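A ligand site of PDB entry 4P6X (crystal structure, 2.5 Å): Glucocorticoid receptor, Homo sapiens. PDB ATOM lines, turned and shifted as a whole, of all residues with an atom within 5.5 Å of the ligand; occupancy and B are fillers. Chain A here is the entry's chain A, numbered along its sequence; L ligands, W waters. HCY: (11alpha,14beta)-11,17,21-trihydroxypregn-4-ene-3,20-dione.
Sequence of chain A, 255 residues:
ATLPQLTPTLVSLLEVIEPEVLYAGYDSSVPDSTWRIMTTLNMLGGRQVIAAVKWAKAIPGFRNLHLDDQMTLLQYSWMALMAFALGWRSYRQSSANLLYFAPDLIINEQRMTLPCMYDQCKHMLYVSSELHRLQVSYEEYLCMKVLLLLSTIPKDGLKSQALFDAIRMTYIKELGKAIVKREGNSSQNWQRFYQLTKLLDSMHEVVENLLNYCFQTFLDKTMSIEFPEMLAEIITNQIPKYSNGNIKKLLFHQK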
ATOM      1  N   MET A  38       6.416 -18.333  -3.073  1.00  0.00           N
ATOM      2  CA  MET A  38       7.392 -19.368  -2.778  1.00  0.00           C
ATOM      3  C   MET A  38       8.077 -19.117  -1.436  1.00  0.00           C
ATOM      4  O   MET A  38       8.178 -20.018  -0.607  1.00  0.00           O
ATOM      5  CB  MET A  38       8.427 -19.462  -3.888  1.00  0.00           C
ATOM      6  CG  MET A  38       7.830 -19.408  -5.279  1.00  0.00           C
ATOM      7  SD  MET A  38       8.222 -20.818  -6.329  1.00  0.00           S
ATOM      8  CE  MET A  38       9.969 -20.593  -6.595  1.00  0.00           C
ATOM      9  N   LEU A  41       5.745 -19.808   1.311  1.00  0.00           N
ATOM     10  CA  LEU A  41       5.551 -21.248   1.429  1.00  0.00           C
ATOM     11  C   LEU A  41       6.728 -21.913   2.146  1.00  0.00           C
ATOM     12  O   LEU A  41       6.528 -22.729   3.052  1.00  0.00           O
ATOM     13  CB  LEU A  41       5.347 -21.879   0.055  1.00  0.00           C
ATOM     14  CG  LEU A  41       4.077 -21.421  -0.666  1.00  0.00           C
ATOM     15  CD1 LEU A  41       3.950 -22.084  -2.032  1.00  0.00           C
ATOM     16  CD2 LEU A  41       2.849 -21.701   0.185  1.00  0.00           C
ATOM     17  N   ASN A  42       7.948 -21.554   1.744  1.00  0.00           N
ATOM     18  CA  ASN A  42       9.146 -22.020   2.438  1.00  0.00           C
ATOM     19  C   ASN A  42       9.070 -21.725   3.927  1.00  0.00           C
ATOM     20  O   ASN A  42       9.363 -22.583   4.760  1.00  0.00           O
ATOM     21  CB  ASN A  42      10.398 -21.360   1.861  1.00  0.00           C
ATOM     22  CG  ASN A  42      10.851 -22.011   0.574  1.00  0.00           C
ATOM     23  OD1 ASN A  42      10.558 -23.172   0.321  1.00  0.00           O
ATOM     24  ND2 ASN A  42      11.594 -21.270  -0.228  1.00  0.00           N
ATOM     25  N   LEU A  44       6.350 -21.215   5.595  1.00  0.00           N
ATOM     26  CA  LEU A  44       5.301 -22.119   6.039  1.00  0.00           C
ATOM     27  C   LEU A  44       5.887 -23.506   6.218  1.00  0.00           C
ATOM     28  O   LEU A  44       5.695 -24.146   7.272  1.00  0.00           O
ATOM     29  CB  LEU A  44       4.153 -22.138   5.039  1.00  0.00           C
ATOM     30  CG  LEU A  44       3.060 -23.202   5.228  1.00  0.00           C
ATOM     31  CD1 LEU A  44       2.411 -23.071   6.601  1.00  0.00           C
ATOM     32  CD2 LEU A  44       2.028 -23.120   4.123  1.00  0.00           C
ATOM     33  N   GLY A  45       6.612 -23.966   5.197  1.00  0.00           N
ATOM     34  CA  GLY A  45       7.243 -25.260   5.216  1.00  0.00           C
ATOM     35  C   GLY A  45       8.100 -25.501   6.442  1.00  0.00           C
ATOM     36  O   GLY A  45       8.044 -26.566   7.045  1.00  0.00           O
ATOM     37  N   GLN A  48       5.769 -26.208   9.289  1.00  0.00           N
ATOM     38  CA  GLN A  48       5.152 -27.524   9.122  1.00  0.00           C
ATOM     39  C   GLN A  48       6.119 -28.636   9.499  1.00  0.00           C
ATOM     40  O   GLN A  48       5.726 -29.616  10.144  1.00  0.00           O
ATOM     41  CB  GLN A  48       4.666 -27.727   7.678  1.00  0.00           C
ATOM     42  CG  GLN A  48       3.471 -26.877   7.293  1.00  0.00           C
ATOM     43  CD  GLN A  48       3.032 -27.130   5.871  1.00  0.00           C
ATOM     44  OE1 GLN A  48       2.228 -26.382   5.317  1.00  0.00           O
ATOM     45  NE2 GLN A  48       3.569 -28.177   5.272  1.00  0.00           N
ATOM     46  N   TRP A  78      11.065 -35.351   4.618  1.00  0.00           N
ATOM     47  CA  TRP A  78      10.285 -34.156   4.966  1.00  0.00           C
ATOM     48  C   TRP A  78       9.502 -33.647   3.763  1.00  0.00           C
ATOM     49  O   TRP A  78       8.350 -33.238   3.892  1.00  0.00           O
ATOM     50  CB  TRP A  78      11.180 -33.044   5.534  1.00  0.00           C
ATOM     51  CG  TRP A  78      12.081 -32.387   4.543  1.00  0.00           C
ATOM     52  CD1 TRP A  78      13.330 -32.779   4.186  1.00  0.00           C
ATOM     53  CD2 TRP A  78      11.801 -31.207   3.782  1.00  0.00           C
ATOM     54  NE1 TRP A  78      13.850 -31.925   3.254  1.00  0.00           N
ATOM     55  CE2 TRP A  78      12.922 -30.941   2.982  1.00  0.00           C
ATOM     56  CE3 TRP A  78      10.700 -30.338   3.700  1.00  0.00           C
ATOM     57  CZ2 TRP A  78      12.991 -29.858   2.109  1.00  0.00           C
ATOM     58  CZ3 TRP A  78      10.769 -29.265   2.827  1.00  0.00           C
ATOM     59  CH2 TRP A  78      11.910 -29.039   2.050  1.00  0.00           C
ATOM     60  N   MET A  79      10.128 -33.669   2.583  1.00  0.00           N
ATOM     61  CA  MET A  79       9.448 -33.254   1.362  1.00  0.00           C
ATOM     62  C   MET A  79       8.278 -34.184   1.058  1.00  0.00           C
ATOM     63  O   MET A  79       7.189 -33.728   0.710  1.00  0.00           O
ATOM     64  CB  MET A  79      10.423 -33.218   0.184  1.00  0.00           C
ATOM     65  CG  MET A  79       9.794 -32.738  -1.104  1.00  0.00           C
ATOM     66  SD  MET A  79       9.200 -31.037  -0.963  1.00  0.00           S
ATOM     67  CE  MET A  79      10.711 -30.115  -1.277  1.00  0.00           C
ATOM     68  N   MET A  82       5.471 -33.330   3.456  1.00  0.00           N
ATOM     69  CA  MET A  82       4.850 -32.070   3.099  1.00  0.00           C
ATOM     70  C   MET A  82       4.023 -32.152   1.829  1.00  0.00           C
ATOM     71  O   MET A  82       2.886 -31.691   1.786  1.00  0.00           O
ATOM     72  CB  MET A  82       5.915 -30.983   2.980  1.00  0.00           C
ATOM     73  CG  MET A  82       5.981 -30.034   4.179  1.00  0.00           C
ATOM     74  SD  MET A  82       6.129 -30.783   5.815  1.00  0.00           S
ATOM     75  CE  MET A  82       4.421 -31.161   6.271  1.00  0.00           C
ATOM     76  N   ALA A  83       4.593 -32.767   0.794  1.00  0.00           N
ATOM     77  CA  ALA A  83       3.905 -32.895  -0.489  1.00  0.00           C
ATOM     78  C   ALA A  83       2.643 -33.745  -0.371  1.00  0.00           C
ATOM     79  O   ALA A  83       1.598 -33.398  -0.892  1.00  0.00           O
ATOM     80  CB  ALA A  83       4.845 -33.484  -1.528  1.00  0.00           C
ATOM     81  N   LEU A  86      -0.014 -32.149   1.457  1.00  0.00           N
ATOM     82  CA  LEU A  86      -0.505 -31.085   0.597  1.00  0.00           C
ATOM     83  C   LEU A  86      -1.746 -31.570  -0.136  1.00  0.00           C
ATOM     84  O   LEU A  86      -2.797 -30.938  -0.081  1.00  0.00           O
ATOM     85  CB  LEU A  86       0.559 -30.625  -0.402  1.00  0.00           C
ATOM     86  CG  LEU A  86       0.198 -29.468  -1.324  1.00  0.00           C
ATOM     87  CD1 LEU A  86      -0.131 -28.231  -0.536  1.00  0.00           C
ATOM     88  CD2 LEU A  86       1.326 -29.189  -2.287  1.00  0.00           C
ATOM     89  N   ARG A  89      -4.943 -32.002   2.050  1.00  0.00           N
ATOM     90  CA  ARG A  89      -5.623 -30.762   2.366  1.00  0.00           C
ATOM     91  C   ARG A  89      -6.385 -30.263   1.157  1.00  0.00           C
ATOM     92  O   ARG A  89      -7.538 -29.895   1.273  1.00  0.00           O
ATOM     93  CB  ARG A  89      -4.638 -29.697   2.844  1.00  0.00           C
ATOM     94  CG  ARG A  89      -4.222 -29.842   4.290  1.00  0.00           C
ATOM     95  CD  ARG A  89      -3.472 -28.619   4.763  1.00  0.00           C
ATOM     96  NE  ARG A  89      -2.549 -28.134   3.736  1.00  0.00           N
ATOM     97  CZ  ARG A  89      -1.331 -28.638   3.540  1.00  0.00           C
ATOM     98  NH1 ARG A  89      -0.888 -29.625   4.291  1.00  0.00           N
ATOM     99  NH2 ARG A  89      -0.563 -28.136   2.585  1.00  0.00           N
ATOM    100  N   PHE A 101      -2.440 -24.955   0.816  1.00  0.00           N
ATOM    101  CA  PHE A 101      -1.284 -24.910   1.709  1.00  0.00           C
ATOM    102  C   PHE A 101      -1.698 -24.546   3.127  1.00  0.00           C
ATOM    103  O   PHE A 101      -1.202 -25.104   4.108  1.00  0.00           O
ATOM    104  CB  PHE A 101      -0.246 -23.908   1.205  1.00  0.00           C
ATOM    105  CG  PHE A 101       0.464 -24.337  -0.058  1.00  0.00           C
ATOM    106  CD1 PHE A 101      -0.006 -23.951  -1.294  1.00  0.00           C
ATOM    107  CD2 PHE A 101       1.603 -25.118   0.012  1.00  0.00           C
ATOM    108  CE1 PHE A 101       0.642 -24.343  -2.452  1.00  0.00           C
ATOM    109  CE2 PHE A 101       2.258 -25.500  -1.139  1.00  0.00           C
ATOM    110  CZ  PHE A 101       1.782 -25.113  -2.368  1.00  0.00           C
ATOM    111  N   GLN A 120       6.056 -25.728 -10.968  1.00  0.00           N
ATOM    112  CA  GLN A 120       6.269 -26.528  -9.769  1.00  0.00           C
ATOM    113  C   GLN A 120       4.975 -27.025  -9.149  1.00  0.00           C
ATOM    114  O   GLN A 120       4.884 -28.198  -8.781  1.00  0.00           O
ATOM    115  CB  GLN A 120       7.064 -25.733  -8.741  1.00  0.00           C
ATOM    116  CG  GLN A 120       8.507 -25.473  -9.141  1.00  0.00           C
ATOM    117  CD  GLN A 120       9.227 -24.596  -8.136  1.00  0.00           C
ATOM    118  OE1 GLN A 120      10.330 -24.919  -7.702  1.00  0.00           O
ATOM    119  NE2 GLN A 120       8.614 -23.477  -7.773  1.00  0.00           N
ATOM    120  N   MET A 124       2.896 -31.344  -7.430  1.00  0.00           N
ATOM    121  CA  MET A 124       2.108 -31.294  -6.214  1.00  0.00           C
ATOM    122  C   MET A 124       0.656 -31.652  -6.489  1.00  0.00           C
ATOM    123  O   MET A 124       0.116 -32.590  -5.908  1.00  0.00           O
ATOM    124  CB  MET A 124       2.199 -29.919  -5.585  1.00  0.00           C
ATOM    125  CG  MET A 124       3.605 -29.505  -5.219  1.00  0.00           C
ATOM    126  SD  MET A 124       3.687 -27.801  -4.625  1.00  0.00           S
ATOM    127  CE  MET A 124       4.962 -27.152  -5.697  1.00  0.00           C
ATOM    128  N   LEU A 210      10.442 -32.332  -6.916  1.00  0.00           N
ATOM    129  CA  LEU A 210      10.229 -31.224  -5.976  1.00  0.00           C
ATOM    130  C   LEU A 210      11.515 -30.850  -5.246  1.00  0.00           C
ATOM    131  O   LEU A 210      11.703 -29.690  -4.871  1.00  0.00           O
ATOM    132  CB  LEU A 210       9.141 -31.582  -4.967  1.00  0.00           C
ATOM    133  CG  LEU A 210       7.728 -31.783  -5.511  1.00  0.00           C
ATOM    134  CD1 LEU A 210       6.745 -32.000  -4.368  1.00  0.00           C
ATOM    135  CD2 LEU A 210       7.318 -30.622  -6.383  1.00  0.00           C
ATOM    136  N   TYR A 213      14.165 -28.785  -7.409  1.00  0.00           N
ATOM    137  CA  TYR A 213      13.691 -27.410  -7.532  1.00  0.00           C
ATOM    138  C   TYR A 213      13.822 -26.669  -6.212  1.00  0.00           C
ATOM    139  O   TYR A 213      14.058 -25.464  -6.172  1.00  0.00           O
ATOM    140  CB  TYR A 213      12.252 -27.378  -8.036  1.00  0.00           C
ATOM    141  CG  TYR A 213      12.111 -27.823  -9.475  1.00  0.00           C
ATOM    142  CD1 TYR A 213      12.612 -27.054 -10.516  1.00  0.00           C
ATOM    143  CD2 TYR A 213      11.462 -29.014  -9.794  1.00  0.00           C
ATOM    144  CE1 TYR A 213      12.487 -27.474 -11.828  1.00  0.00           C
ATOM    145  CE2 TYR A 213      11.344 -29.445 -11.099  1.00  0.00           C
ATOM    146  CZ  TYR A 213      11.853 -28.665 -12.120  1.00  0.00           C
ATOM    147  OH  TYR A 213      11.720 -29.085 -13.425  1.00  0.00           O
ATOM    148  N   CYS A 214      13.668 -27.409  -5.111  1.00  0.00           N
ATOM    149  CA  CYS A 214      13.933 -26.863  -3.785  1.00  0.00           C
ATOM    150  C   CYS A 214      15.406 -26.474  -3.716  1.00  0.00           C
ATOM    151  O   CYS A 214      15.747 -25.394  -3.226  1.00  0.00           O
ATOM    152  CB  CYS A 214      13.599 -27.886  -2.685  1.00  0.00           C
ATOM    153  SG  CYS A 214      14.063 -27.383  -1.004  1.00  0.00           S
ATOM    154  N   THR A 217      16.192 -23.270  -6.184  1.00  0.00           N
ATOM    155  CA  THR A 217      15.783 -22.009  -5.602  1.00  0.00           C
ATOM    156  C   THR A 217      16.642 -21.649  -4.379  1.00  0.00           C
ATOM    157  O   THR A 217      16.745 -20.486  -4.004  1.00  0.00           O
ATOM    158  CB  THR A 217      14.314 -22.028  -5.191  1.00  0.00           C
ATOM    159  OG1 THR A 217      14.084 -23.093  -4.267  1.00  0.00           O
ATOM    160  CG2 THR A 217      13.426 -22.237  -6.426  1.00  0.00           C
ATOM    161  N   ILE A 225      13.614 -15.881  -3.703  1.00  0.00           N
ATOM    162  CA  ILE A 225      13.147 -16.864  -2.724  1.00  0.00           C
ATOM    163  C   ILE A 225      14.069 -17.069  -1.521  1.00  0.00           C
ATOM    164  O   ILE A 225      15.245 -17.378  -1.661  1.00  0.00           O
ATOM    165  CB  ILE A 225      12.942 -18.227  -3.409  1.00  0.00           C
ATOM    166  CG1 ILE A 225      12.231 -18.026  -4.741  1.00  0.00           C
ATOM    167  CG2 ILE A 225      12.185 -19.173  -2.506  1.00  0.00           C
ATOM    168  CD1 ILE A 225      12.800 -18.854  -5.845  1.00  0.00           C
ATOM    169  N   PHE A 227      14.569 -18.934   2.486  1.00  0.00           N
ATOM    170  CA  PHE A 227      14.193 -20.077   3.315  1.00  0.00           C
ATOM    171  C   PHE A 227      14.393 -19.783   4.794  1.00  0.00           C
ATOM    172  O   PHE A 227      15.308 -19.050   5.173  1.00  0.00           O
ATOM    173  CB  PHE A 227      15.015 -21.315   2.941  1.00  0.00           C
ATOM    174  CG  PHE A 227      14.758 -21.824   1.549  1.00  0.00           C
ATOM    175  CD1 PHE A 227      15.318 -21.190   0.448  1.00  0.00           C
ATOM    176  CD2 PHE A 227      13.978 -22.955   1.348  1.00  0.00           C
ATOM    177  CE1 PHE A 227      15.085 -21.664  -0.825  1.00  0.00           C
ATOM    178  CE2 PHE A 227      13.752 -23.441   0.068  1.00  0.00           C
ATOM    179  CZ  PHE A 227      14.312 -22.796  -1.019  1.00  0.00           C
ATOM    180  N   LEU A 231      14.506 -25.129   7.597  1.00  0.00           N
ATOM    181  CA  LEU A 231      14.615 -25.729   6.276  1.00  0.00           C
ATOM    182  C   LEU A 231      16.024 -25.593   5.726  1.00  0.00           C
ATOM    183  O   LEU A 231      16.550 -26.529   5.122  1.00  0.00           O
ATOM    184  CB  LEU A 231      13.612 -25.091   5.311  1.00  0.00           C
ATOM    185  CG  LEU A 231      12.416 -25.955   4.891  1.00  0.00           C
ATOM    186  CD1 LEU A 231      11.974 -26.863   6.029  1.00  0.00           C
ATOM    187  CD2 LEU A 231      11.262 -25.101   4.421  1.00  0.00           C
HETATM  188  C1  HCY L   1       5.455 -25.814   1.873  1.00  0.00           C
HETATM  189  C2  HCY L   1       4.281 -26.184   2.770  1.00  0.00           C
HETATM  190  C3  HCY L   1       3.388 -27.219   2.113  1.00  0.00           C
HETATM  191  C4  HCY L   1       3.913 -28.104   1.069  1.00  0.00           C
HETATM  192  C5  HCY L   1       5.165 -27.999   0.607  1.00  0.00           C
HETATM  193  C6  HCY L   1       5.614 -29.038  -0.388  1.00  0.00           C
HETATM  194  C7  HCY L   1       6.322 -28.402  -1.554  1.00  0.00           C
HETATM  195  C8  HCY L   1       7.314 -27.320  -1.141  1.00  0.00           C
HETATM  196  C9  HCY L   1       6.744 -26.286  -0.166  1.00  0.00           C
HETATM  197  C10 HCY L   1       6.136 -26.933   1.098  1.00  0.00           C
HETATM  198  C12 HCY L   1       8.225 -24.492  -1.209  1.00  0.00           C
HETATM  199  C11 HCY L   1       7.683 -25.078   0.101  1.00  0.00           C
HETATM  200  C13 HCY L   1       8.787 -25.525  -2.191  1.00  0.00           C
HETATM  201  C14 HCY L   1       7.727 -26.596  -2.406  1.00  0.00           C
HETATM  202  C15 HCY L   1       8.309 -27.445  -3.509  1.00  0.00           C
HETATM  203  C16 HCY L   1       9.109 -26.478  -4.370  1.00  0.00           C
HETATM  204  C17 HCY L   1       9.051 -25.145  -3.674  1.00  0.00           C
HETATM  205  C18 HCY L   1      10.072 -26.119  -1.613  1.00  0.00           C
HETATM  206  C19 HCY L   1       7.191 -27.657   1.953  1.00  0.00           C
HETATM  207  C20 HCY L   1      10.317 -24.343  -3.967  1.00  0.00           C
HETATM  208  C21 HCY L   1      10.367 -22.933  -3.495  1.00  0.00           C
HETATM  209  O1  HCY L   1       2.219 -27.333   2.447  1.00  0.00           O
HETATM  210  O2  HCY L   1       8.770 -25.341   1.008  1.00  0.00           O
HETATM  211  O3  HCY L   1       7.942 -24.427  -4.245  1.00  0.00           O
HETATM  212  O4  HCY L   1      11.271 -24.833  -4.551  1.00  0.00           O
HETATM  213  O5  HCY L   1      11.645 -22.381  -3.770  1.00  0.00           O
HETATM  214  O   HOH W   1       1.926 -30.120   3.570  1.00  0.00           O
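NE2 of Gln 48 lies close to SD of Met 82 (3.7 Å).
The side-chain hydroxyl of Thr 217 sits at hydrogen-bond distance from the backbone carbonyl oxygen of Tyr 213 (3.0 Å).
NE2 of Gln 120 sits at hydrogen-bond distance from SD of Met 38 (3.1 Å).
OG1 of Thr 217 is in hydrogen-bond range of O of Cys 214, 3.0 Å away.
The guanidinium group (NE) of Arg 89 sits at hydrogen-bond distance from the backbone carbonyl oxygen (O) of Phe 101.
Water W1 lies within hydrogen-bond range of O of Met 82, NH1 of Arg 89, O1 of the ligand and NE2 of Gln 48.
OD1 of Asn 42 lies within hydrogen-bond range of O2 of the ligand, at 2.9 Å.
O5 of the ligand sits at hydrogen-bond distance from OG1 of Thr 217, at 2.6 Å.
NH2 of Arg 89 lies within hydrogen-bond range of O1 of the ligand, 2.9 Å away.
OE1 of Gln 120 lies close to O4 of the ligand, at 3.3 Å.
The side-chain amide oxygen of Gln 48 sits close to an oxygen (O1) of the ligand (3.0 Å).
An oxygen (O4) of the ligand lies close to the backbone carbonyl oxygen (O) of Tyr 213.
Residues that only touch the ligand: Met 38, Leu 41, Gly 45, Met 79, Met 82, Leu 86, Phe 101, Cys 214, Ile 225 and Phe 227.
Within 4 Å of the ligand: Met 38, Leu 41, Asn 42, Gly 45, Gln 48, Met 79, Met 82, Leu 86, Arg 89, Phe 101, Gln 120, Tyr 213, Cys 214, Thr 217, Ile 225 and Phe 227.
The nearest printed residue that does not touch the ligand is Met 124 (4.01 Å).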
